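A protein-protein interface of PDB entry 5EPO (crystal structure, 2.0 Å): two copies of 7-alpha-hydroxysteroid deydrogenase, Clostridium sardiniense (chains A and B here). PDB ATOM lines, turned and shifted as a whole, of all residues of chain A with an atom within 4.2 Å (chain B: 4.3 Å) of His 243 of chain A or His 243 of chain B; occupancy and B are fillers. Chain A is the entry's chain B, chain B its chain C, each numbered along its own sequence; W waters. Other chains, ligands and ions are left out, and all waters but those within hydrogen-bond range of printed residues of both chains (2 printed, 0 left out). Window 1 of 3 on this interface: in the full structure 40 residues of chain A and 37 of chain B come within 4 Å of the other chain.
Tyr 229 of chain B touches Ala 226 of chain A. Ala 226 of chain B touches Tyr 229 of chain A (CB to OH, 3.7 Å). His 243 of chain B touches Tyr 230 of chain A. CE of Met 241 of chain A touches CE of Met 241 of chain B, 3.4 Å away. Met 241 of chain A touches Ile 242 of chain B (CE to O, 3.5 Å). Met 241 of chain A touches His 243 of chain B (CE to CA, 3.9 Å). CE of Met 241 of chain B touches O of Ile 242 of chain A, at 3.5 Å. Tyr 230 of chain B touches His 243 of chain A. His 243 of chain A touches His 243 of chain B (ND1 to ND1, 3.9 Å).
Hydrophobic or aromatic side chains of chain B within 4 Å of the printed part of chain A: Ala 226, Tyr 229, Tyr 230, Met 241 and His 243. Along chain B the printed residues that touch a printed residue of chain A span positions 226 to 244. Hydrophobic or aromatic side chains of chain A that line the printed part of chain B: Ala 226, Tyr 229, Tyr 230, Met 241 and His 243.
N of Ala 185 of chain A is in hydrogen-bond range of O of Met 241 of chain A, at 2.9 Å. The backbone carbonyl oxygen (O) of Ala 185 of chain A lies within hydrogen-bond range of the backbone NH (N) of His 243 of chain A (2.8 Å). OH of Tyr 230 of chain A lies within hydrogen-bond range of ND1 of His 243 of chain A, 2.8 Å away. N of Ala 185 of chain B lies within hydrogen-bond range of O of Met 241 of chain B, 2.8 Å away. N of His 243 of chain B lies within hydrogen-bond range of O of Ala 185 of chain B, 2.8 Å away. O of His 243 of chain B sits at hydrogen-bond distance from N of Leu 187 of chain B, 2.7 Å away.
Water W1 lies within hydrogen-bond range of the side-chain carboxylate of Glu 244 of chain A and the side-chain sulfur of Met 241 of chain B. Water W2 bridges OE1 of Glu 244 of chain B and SD of Met 241 of chain A.
The side-chain hydroxyl (OH) of Tyr 229 of chain A lies within hydrogen-bond range of a ring nitrogen (NE2) of His 243 of chain B. The side-chain sulfur (SD) of Met 241 of chain A lies within hydrogen-bond range of the backbone NH (N) of Glu 244 of chain B (3.4 Å). A ring nitrogen (NE2) of His 243 of chain A lies within hydrogen-bond range of the side-chain hydroxyl (OH) of Tyr 229 of chain B, 3.0 Å away. N of Glu 244 of chain A is in hydrogen-bond range of SD of Met 241 of chain B (3.5 Å).
Ala 226 of chain A touches Tyr 229 of chain B, and with the chains exchanged Tyr 229 of chain A touches Ala 226 of chain B. Met 241 of chain A touches Ile 242 of chain B, and with the chains exchanged Ile 242 of chain A touches Met 241 of chain B. Met 241 of chain A touches Glu 244 of chain B, and with the chains exchanged Glu 244 of chain A touches Met 241 of chain B. His 243 of chain A touches its own counterpart, His 243 of chain B. Positions printed for both chains: 185, 186, 187, 226, 229, 230, 241, 242, 243, 244 and 245. Of the 13 pairs that touch across the chains among the printed residues, 12 have their exchanged pair printed and touching as well.
Leu 187 of chain A touches none of the printed residues of chain B. Printed residues of chain B within 4 Å of Tyr 229 of chain A: Ala 226 (3.7 Å) and His 243 (2.8 Å). Of the printed residues of chain B, Glu 244 of chain A touches Met 241 (3.5 Å). Printed residues of chain A within 4 Å of Tyr 230 of chain B: His 243 (3.4 Å). His 243 of chain B touches just these residues of chain A: Tyr 229 (2.8 Å), Tyr 230 (3.3 Å), Met 241 (3.9 Å) and His 243 (3.9 Å). Of the printed residues of chain A, Glu 244 of chain B touches Met 241 (3.4 Å). The nearest printed residue of chain B that does not touch His 243 of chain A is Met 241 of chain B (4.001 Å).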
ATOM      1  N   ALA A 185     -10.093  35.073  -4.548  1.00  0.00           N
ATOM      2  CA  ALA A 185      -9.137  35.281  -3.504  1.00  0.00           C
ATOM      3  C   ALA A 185      -8.551  33.975  -2.987  1.00  0.00           C
ATOM      4  O   ALA A 185      -9.264  33.006  -2.767  1.00  0.00           O
ATOM      5  CB  ALA A 185      -9.778  36.062  -2.347  1.00  0.00           C
ATOM      6  N   VAL A 186      -7.235  33.983  -2.800  1.00  0.00           N
ATOM      7  CA  VAL A 186      -6.504  32.834  -2.255  1.00  0.00           C
ATOM      8  C   VAL A 186      -6.006  33.197  -0.855  1.00  0.00           C
ATOM      9  O   VAL A 186      -5.389  34.247  -0.659  1.00  0.00           O
ATOM     10  CB  VAL A 186      -5.330  32.458  -3.154  1.00  0.00           C
ATOM     11  CG1 VAL A 186      -4.490  31.372  -2.539  1.00  0.00           C
ATOM     12  CG2 VAL A 186      -5.832  31.991  -4.519  1.00  0.00           C
ATOM     13  N   LEU A 187      -6.318  32.346   0.119  1.00  0.00           N
ATOM     14  CA  LEU A 187      -6.087  32.652   1.549  1.00  0.00           C
ATOM     15  C   LEU A 187      -5.044  31.671   2.109  1.00  0.00           C
ATOM     16  O   LEU A 187      -5.376  30.567   2.542  1.00  0.00           O
ATOM     17  CB  LEU A 187      -7.366  32.510   2.360  1.00  0.00           C
ATOM     18  CG  LEU A 187      -8.434  33.577   2.284  1.00  0.00           C
ATOM     19  CD1 LEU A 187      -8.902  33.826   0.866  1.00  0.00           C
ATOM     20  CD2 LEU A 187      -9.612  33.194   3.154  1.00  0.00           C
ATOM     21  N   ALA A 226      -2.565  27.309  -6.594  1.00  0.00           N
ATOM     22  CA  ALA A 226      -3.942  27.826  -6.578  1.00  0.00           C
ATOM     23  C   ALA A 226      -4.033  29.045  -7.494  1.00  0.00           C
ATOM     24  O   ALA A 226      -5.026  29.202  -8.218  1.00  0.00           O
ATOM     25  CB  ALA A 226      -4.356  28.227  -5.161  1.00  0.00           C
ATOM     26  N   TYR A 229      -4.365  27.930 -11.095  1.00  0.00           N
ATOM     27  CA  TYR A 229      -5.745  27.471 -11.347  1.00  0.00           C
ATOM     28  C   TYR A 229      -6.661  28.673 -11.663  1.00  0.00           C
ATOM     29  O   TYR A 229      -7.333  28.696 -12.680  1.00  0.00           O
ATOM     30  CB  TYR A 229      -6.278  26.666 -10.127  1.00  0.00           C
ATOM     31  CG  TYR A 229      -7.766  26.347 -10.196  1.00  0.00           C
ATOM     32  CD1 TYR A 229      -8.224  25.330 -11.011  1.00  0.00           C
ATOM     33  CD2 TYR A 229      -8.699  27.074  -9.471  1.00  0.00           C
ATOM     34  CE1 TYR A 229      -9.592  25.037 -11.101  1.00  0.00           C
ATOM     35  CE2 TYR A 229     -10.042  26.786  -9.550  1.00  0.00           C
ATOM     36  CZ  TYR A 229     -10.484  25.772 -10.371  1.00  0.00           C
ATOM     37  OH  TYR A 229     -11.839  25.487 -10.438  1.00  0.00           O
ATOM     38  N   TYR A 230      -6.631  29.692 -10.797  1.00  0.00           N
ATOM     39  CA  TYR A 230      -7.519  30.828 -10.904  1.00  0.00           C
ATOM     40  C   TYR A 230      -7.160  31.777 -12.052  1.00  0.00           C
ATOM     41  O   TYR A 230      -8.030  32.425 -12.621  1.00  0.00           O
ATOM     42  CB  TYR A 230      -7.585  31.590  -9.572  1.00  0.00           C
ATOM     43  CG  TYR A 230      -8.476  30.904  -8.568  1.00  0.00           C
ATOM     44  CD1 TYR A 230      -9.846  30.831  -8.790  1.00  0.00           C
ATOM     45  CD2 TYR A 230      -7.968  30.293  -7.443  1.00  0.00           C
ATOM     46  CE1 TYR A 230     -10.679  30.186  -7.912  1.00  0.00           C
ATOM     47  CE2 TYR A 230      -8.802  29.638  -6.535  1.00  0.00           C
ATOM     48  CZ  TYR A 230     -10.162  29.569  -6.802  1.00  0.00           C
ATOM     49  OH  TYR A 230     -11.012  28.899  -5.977  1.00  0.00           O
ATOM     50  N   MET A 241     -14.654  33.261  -5.631  1.00  0.00           N
ATOM     51  CA  MET A 241     -14.284  32.249  -4.668  1.00  0.00           C
ATOM     52  C   MET A 241     -13.370  32.794  -3.556  1.00  0.00           C
ATOM     53  O   MET A 241     -12.534  33.681  -3.769  1.00  0.00           O
ATOM     54  CB  MET A 241     -13.595  31.070  -5.326  1.00  0.00           C
ATOM     55  CG  MET A 241     -14.543  29.992  -5.788  1.00  0.00           C
ATOM     56  SD  MET A 241     -15.528  29.197  -4.516  1.00  0.00           S
ATOM     57  CE  MET A 241     -14.268  28.462  -3.526  1.00  0.00           C
ATOM     58  N   ILE A 242     -13.587  32.237  -2.346  1.00  0.00           N
ATOM     59  CA  ILE A 242     -12.699  32.425  -1.238  1.00  0.00           C
ATOM     60  C   ILE A 242     -11.990  31.103  -1.044  1.00  0.00           C
ATOM     61  O   ILE A 242     -12.555  30.151  -0.530  1.00  0.00           O
ATOM     62  CB  ILE A 242     -13.470  32.862   0.056  1.00  0.00           C
ATOM     63  CG1 ILE A 242     -14.370  34.075  -0.240  1.00  0.00           C
ATOM     64  CG2 ILE A 242     -12.501  33.155   1.191  1.00  0.00           C
ATOM     65  CD1 ILE A 242     -13.643  35.297  -0.769  1.00  0.00           C
ATOM     66  N   HIS A 243     -10.730  31.054  -1.453  1.00  0.00           N
ATOM     67  CA  HIS A 243     -10.027  29.787  -1.588  1.00  0.00           C
ATOM     68  C   HIS A 243      -8.975  29.592  -0.495  1.00  0.00           C
ATOM     69  O   HIS A 243      -7.950  30.276  -0.471  1.00  0.00           O
ATOM     70  CB  HIS A 243      -9.418  29.711  -3.004  1.00  0.00           C
ATOM     71  CG  HIS A 243      -8.908  28.366  -3.370  1.00  0.00           C
ATOM     72  ND1 HIS A 243      -9.662  27.453  -4.055  1.00  0.00           N
ATOM     73  CD2 HIS A 243      -7.699  27.789  -3.174  1.00  0.00           C
ATOM     74  CE1 HIS A 243      -8.948  26.353  -4.263  1.00  0.00           C
ATOM     75  NE2 HIS A 243      -7.757  26.522  -3.717  1.00  0.00           N
ATOM     76  N   GLU A 244      -9.233  28.629   0.408  1.00  0.00           N
ATOM     77  CA  GLU A 244      -8.381  28.410   1.567  1.00  0.00           C
ATOM     78  C   GLU A 244      -7.214  27.478   1.263  1.00  0.00           C
ATOM     79  O   GLU A 244      -7.407  26.368   0.826  1.00  0.00           O
ATOM     80  CB  GLU A 244      -9.232  27.860   2.730  1.00  0.00           C
ATOM     81  CG  GLU A 244     -10.306  28.854   3.238  1.00  0.00           C
ATOM     82  CD  GLU A 244     -11.220  28.299   4.309  1.00  0.00           C
ATOM     83  OE1 GLU A 244     -10.943  27.182   4.841  1.00  0.00           O
ATOM     84  OE2 GLU A 244     -12.216  28.959   4.606  1.00  0.00           O
ATOM     85  N   VAL A 245      -6.005  27.946   1.497  1.00  0.00           N
ATOM     86  CA  VAL A 245      -4.824  27.126   1.370  1.00  0.00           C
ATOM     87  C   VAL A 245      -4.013  27.181   2.665  1.00  0.00           C
ATOM     88  O   VAL A 245      -2.965  27.808   2.727  1.00  0.00           O
ATOM     89  CB  VAL A 245      -3.930  27.545   0.196  1.00  0.00           C
ATOM     90  CG1 VAL A 245      -2.898  26.447  -0.089  1.00  0.00           C
ATOM     91  CG2 VAL A 245      -4.768  27.797  -1.044  1.00  0.00           C
ATOM     92  N   ALA B 185     -15.217  19.387  -1.825  1.00  0.00           N
ATOM     93  CA  ALA B 185     -16.447  19.323  -2.637  1.00  0.00           C
ATOM     94  C   ALA B 185     -16.418  20.325  -3.761  1.00  0.00           C
ATOM     95  O   ALA B 185     -16.007  21.483  -3.583  1.00  0.00           O
ATOM     96  CB  ALA B 185     -17.684  19.526  -1.769  1.00  0.00           C
ATOM     97  N   VAL B 186     -16.913  19.885  -4.918  1.00  0.00           N
ATOM     98  CA  VAL B 186     -17.038  20.726  -6.122  1.00  0.00           C
ATOM     99  C   VAL B 186     -18.534  20.875  -6.458  1.00  0.00           C
ATOM    100  O   VAL B 186     -19.244  19.873  -6.687  1.00  0.00           O
ATOM    101  CB  VAL B 186     -16.301  20.089  -7.292  1.00  0.00           C
ATOM    102  CG1 VAL B 186     -16.498  20.941  -8.560  1.00  0.00           C
ATOM    103  CG2 VAL B 186     -14.794  19.957  -6.992  1.00  0.00           C
ATOM    104  N   LEU B 187     -19.004  22.112  -6.481  1.00  0.00           N
ATOM    105  CA  LEU B 187     -20.432  22.399  -6.628  1.00  0.00           C
ATOM    106  C   LEU B 187     -20.739  22.966  -8.024  1.00  0.00           C
ATOM    107  O   LEU B 187     -20.574  24.157  -8.260  1.00  0.00           O
ATOM    108  CB  LEU B 187     -20.858  23.471  -5.577  1.00  0.00           C
ATOM    109  CG  LEU B 187     -20.968  23.044  -4.116  1.00  0.00           C
ATOM    110  CD1 LEU B 187     -19.687  22.406  -3.600  1.00  0.00           C
ATOM    111  CD2 LEU B 187     -21.326  24.239  -3.250  1.00  0.00           C
ATOM    112  N   ALA B 226     -11.734  21.336 -12.016  1.00  0.00           N
ATOM    113  CA  ALA B 226     -11.683  21.469 -10.553  1.00  0.00           C
ATOM    114  C   ALA B 226     -11.358  20.144  -9.885  1.00  0.00           C
ATOM    115  O   ALA B 226     -10.575  20.097  -8.921  1.00  0.00           O
ATOM    116  CB  ALA B 226     -12.982  22.016 -10.010  1.00  0.00           C
ATOM    117  N   TYR B 229      -7.686  19.537 -10.078  1.00  0.00           N
ATOM    118  CA  TYR B 229      -6.974  20.351  -9.105  1.00  0.00           C
ATOM    119  C   TYR B 229      -6.982  19.647  -7.741  1.00  0.00           C
ATOM    120  O   TYR B 229      -5.913  19.470  -7.123  1.00  0.00           O
ATOM    121  CB  TYR B 229      -7.615  21.740  -8.975  1.00  0.00           C
ATOM    122  CG  TYR B 229      -7.079  22.567  -7.825  1.00  0.00           C
ATOM    123  CD1 TYR B 229      -5.805  23.113  -7.883  1.00  0.00           C
ATOM    124  CD2 TYR B 229      -7.813  22.760  -6.684  1.00  0.00           C
ATOM    125  CE1 TYR B 229      -5.294  23.841  -6.856  1.00  0.00           C
ATOM    126  CE2 TYR B 229      -7.333  23.506  -5.621  1.00  0.00           C
ATOM    127  CZ  TYR B 229      -6.063  24.042  -5.691  1.00  0.00           C
ATOM    128  OH  TYR B 229      -5.561  24.768  -4.647  1.00  0.00           O
ATOM    129  N   TYR B 230      -8.164  19.238  -7.301  1.00  0.00           N
ATOM    130  CA  TYR B 230      -8.313  18.663  -5.973  1.00  0.00           C
ATOM    131  C   TYR B 230      -7.738  17.241  -5.871  1.00  0.00           C
ATOM    132  O   TYR B 230      -7.344  16.825  -4.795  1.00  0.00           O
ATOM    133  CB  TYR B 230      -9.794  18.700  -5.525  1.00  0.00           C
ATOM    134  CG  TYR B 230     -10.207  20.081  -5.083  1.00  0.00           C
ATOM    135  CD1 TYR B 230      -9.749  20.603  -3.900  1.00  0.00           C
ATOM    136  CD2 TYR B 230     -11.019  20.877  -5.885  1.00  0.00           C
ATOM    137  CE1 TYR B 230     -10.095  21.868  -3.477  1.00  0.00           C
ATOM    138  CE2 TYR B 230     -11.381  22.162  -5.498  1.00  0.00           C
ATOM    139  CZ  TYR B 230     -10.906  22.660  -4.274  1.00  0.00           C
ATOM    140  OH  TYR B 230     -11.208  23.913  -3.855  1.00  0.00           O
ATOM    141  N   MET B 241     -12.615  22.147   1.391  1.00  0.00           N
ATOM    142  CA  MET B 241     -13.149  23.224   0.575  1.00  0.00           C
ATOM    143  C   MET B 241     -14.517  22.903  -0.012  1.00  0.00           C
ATOM    144  O   MET B 241     -14.799  21.764  -0.393  1.00  0.00           O
ATOM    145  CB  MET B 241     -12.217  23.589  -0.593  1.00  0.00           C
ATOM    146  CG  MET B 241     -11.081  24.519  -0.227  1.00  0.00           C
ATOM    147  SD  MET B 241     -11.655  26.174   0.230  1.00  0.00           S
ATOM    148  CE  MET B 241     -12.553  26.710  -1.192  1.00  0.00           C
ATOM    149  N   ILE B 242     -15.320  23.953  -0.123  1.00  0.00           N
ATOM    150  CA  ILE B 242     -16.601  23.976  -0.841  1.00  0.00           C
ATOM    151  C   ILE B 242     -16.408  24.872  -2.055  1.00  0.00           C
ATOM    152  O   ILE B 242     -16.386  26.126  -1.936  1.00  0.00           O
ATOM    153  CB  ILE B 242     -17.726  24.554   0.034  1.00  0.00           C
ATOM    154  CG1 ILE B 242     -17.772  23.867   1.392  1.00  0.00           C
ATOM    155  CG2 ILE B 242     -19.074  24.479  -0.685  1.00  0.00           C
ATOM    156  CD1 ILE B 242     -17.906  22.381   1.307  1.00  0.00           C
ATOM    157  N   HIS B 243     -16.242  24.247  -3.207  1.00  0.00           N
ATOM    158  CA  HIS B 243     -15.690  24.927  -4.396  1.00  0.00           C
ATOM    159  C   HIS B 243     -16.801  25.132  -5.414  1.00  0.00           C
ATOM    160  O   HIS B 243     -17.288  24.191  -5.975  1.00  0.00           O
ATOM    161  CB  HIS B 243     -14.562  24.093  -4.961  1.00  0.00           C
ATOM    162  CG  HIS B 243     -13.754  24.758  -6.001  1.00  0.00           C
ATOM    163  ND1 HIS B 243     -12.551  25.360  -5.728  1.00  0.00           N
ATOM    164  CD2 HIS B 243     -13.930  24.857  -7.340  1.00  0.00           C
ATOM    165  CE1 HIS B 243     -12.050  25.856  -6.843  1.00  0.00           C
ATOM    166  NE2 HIS B 243     -12.871  25.568  -7.830  1.00  0.00           N
ATOM    167  N   GLU B 244     -17.186  26.389  -5.625  1.00  0.00           N
ATOM    168  CA  GLU B 244     -18.313  26.718  -6.506  1.00  0.00           C
ATOM    169  C   GLU B 244     -17.896  26.865  -7.961  1.00  0.00           C
ATOM    170  O   GLU B 244     -17.017  27.660  -8.290  1.00  0.00           O
ATOM    171  CB  GLU B 244     -18.948  28.020  -6.026  1.00  0.00           C
ATOM    172  CG  GLU B 244     -19.478  27.944  -4.610  1.00  0.00           C
ATOM    173  CD  GLU B 244     -20.112  29.230  -4.137  1.00  0.00           C
ATOM    174  OE1 GLU B 244     -20.302  30.145  -4.975  1.00  0.00           O
ATOM    175  OE2 GLU B 244     -20.434  29.349  -2.940  1.00  0.00           O
ATOM    176  N   VAL B 245     -18.519  26.088  -8.826  1.00  0.00           N
ATOM    177  CA  VAL B 245     -18.250  26.163 -10.265  1.00  0.00           C
ATOM    178  C   VAL B 245     -19.598  26.380 -10.960  1.00  0.00           C
ATOM    179  O   VAL B 245     -20.156  25.451 -11.533  1.00  0.00           O
ATOM    180  CB  VAL B 245     -17.552  24.916 -10.777  1.00  0.00           C
ATOM    181  CG1 VAL B 245     -17.093  25.129 -12.214  1.00  0.00           C
ATOM    182  CG2 VAL B 245     -16.317  24.612  -9.943  1.00  0.00           C
HETATM  183  O   HOH W   1     -10.875  24.539   3.430  1.00  0.00           O
HETATM  184  O   HOH W   2     -17.742  31.674  -6.080  1.00  0.00           O
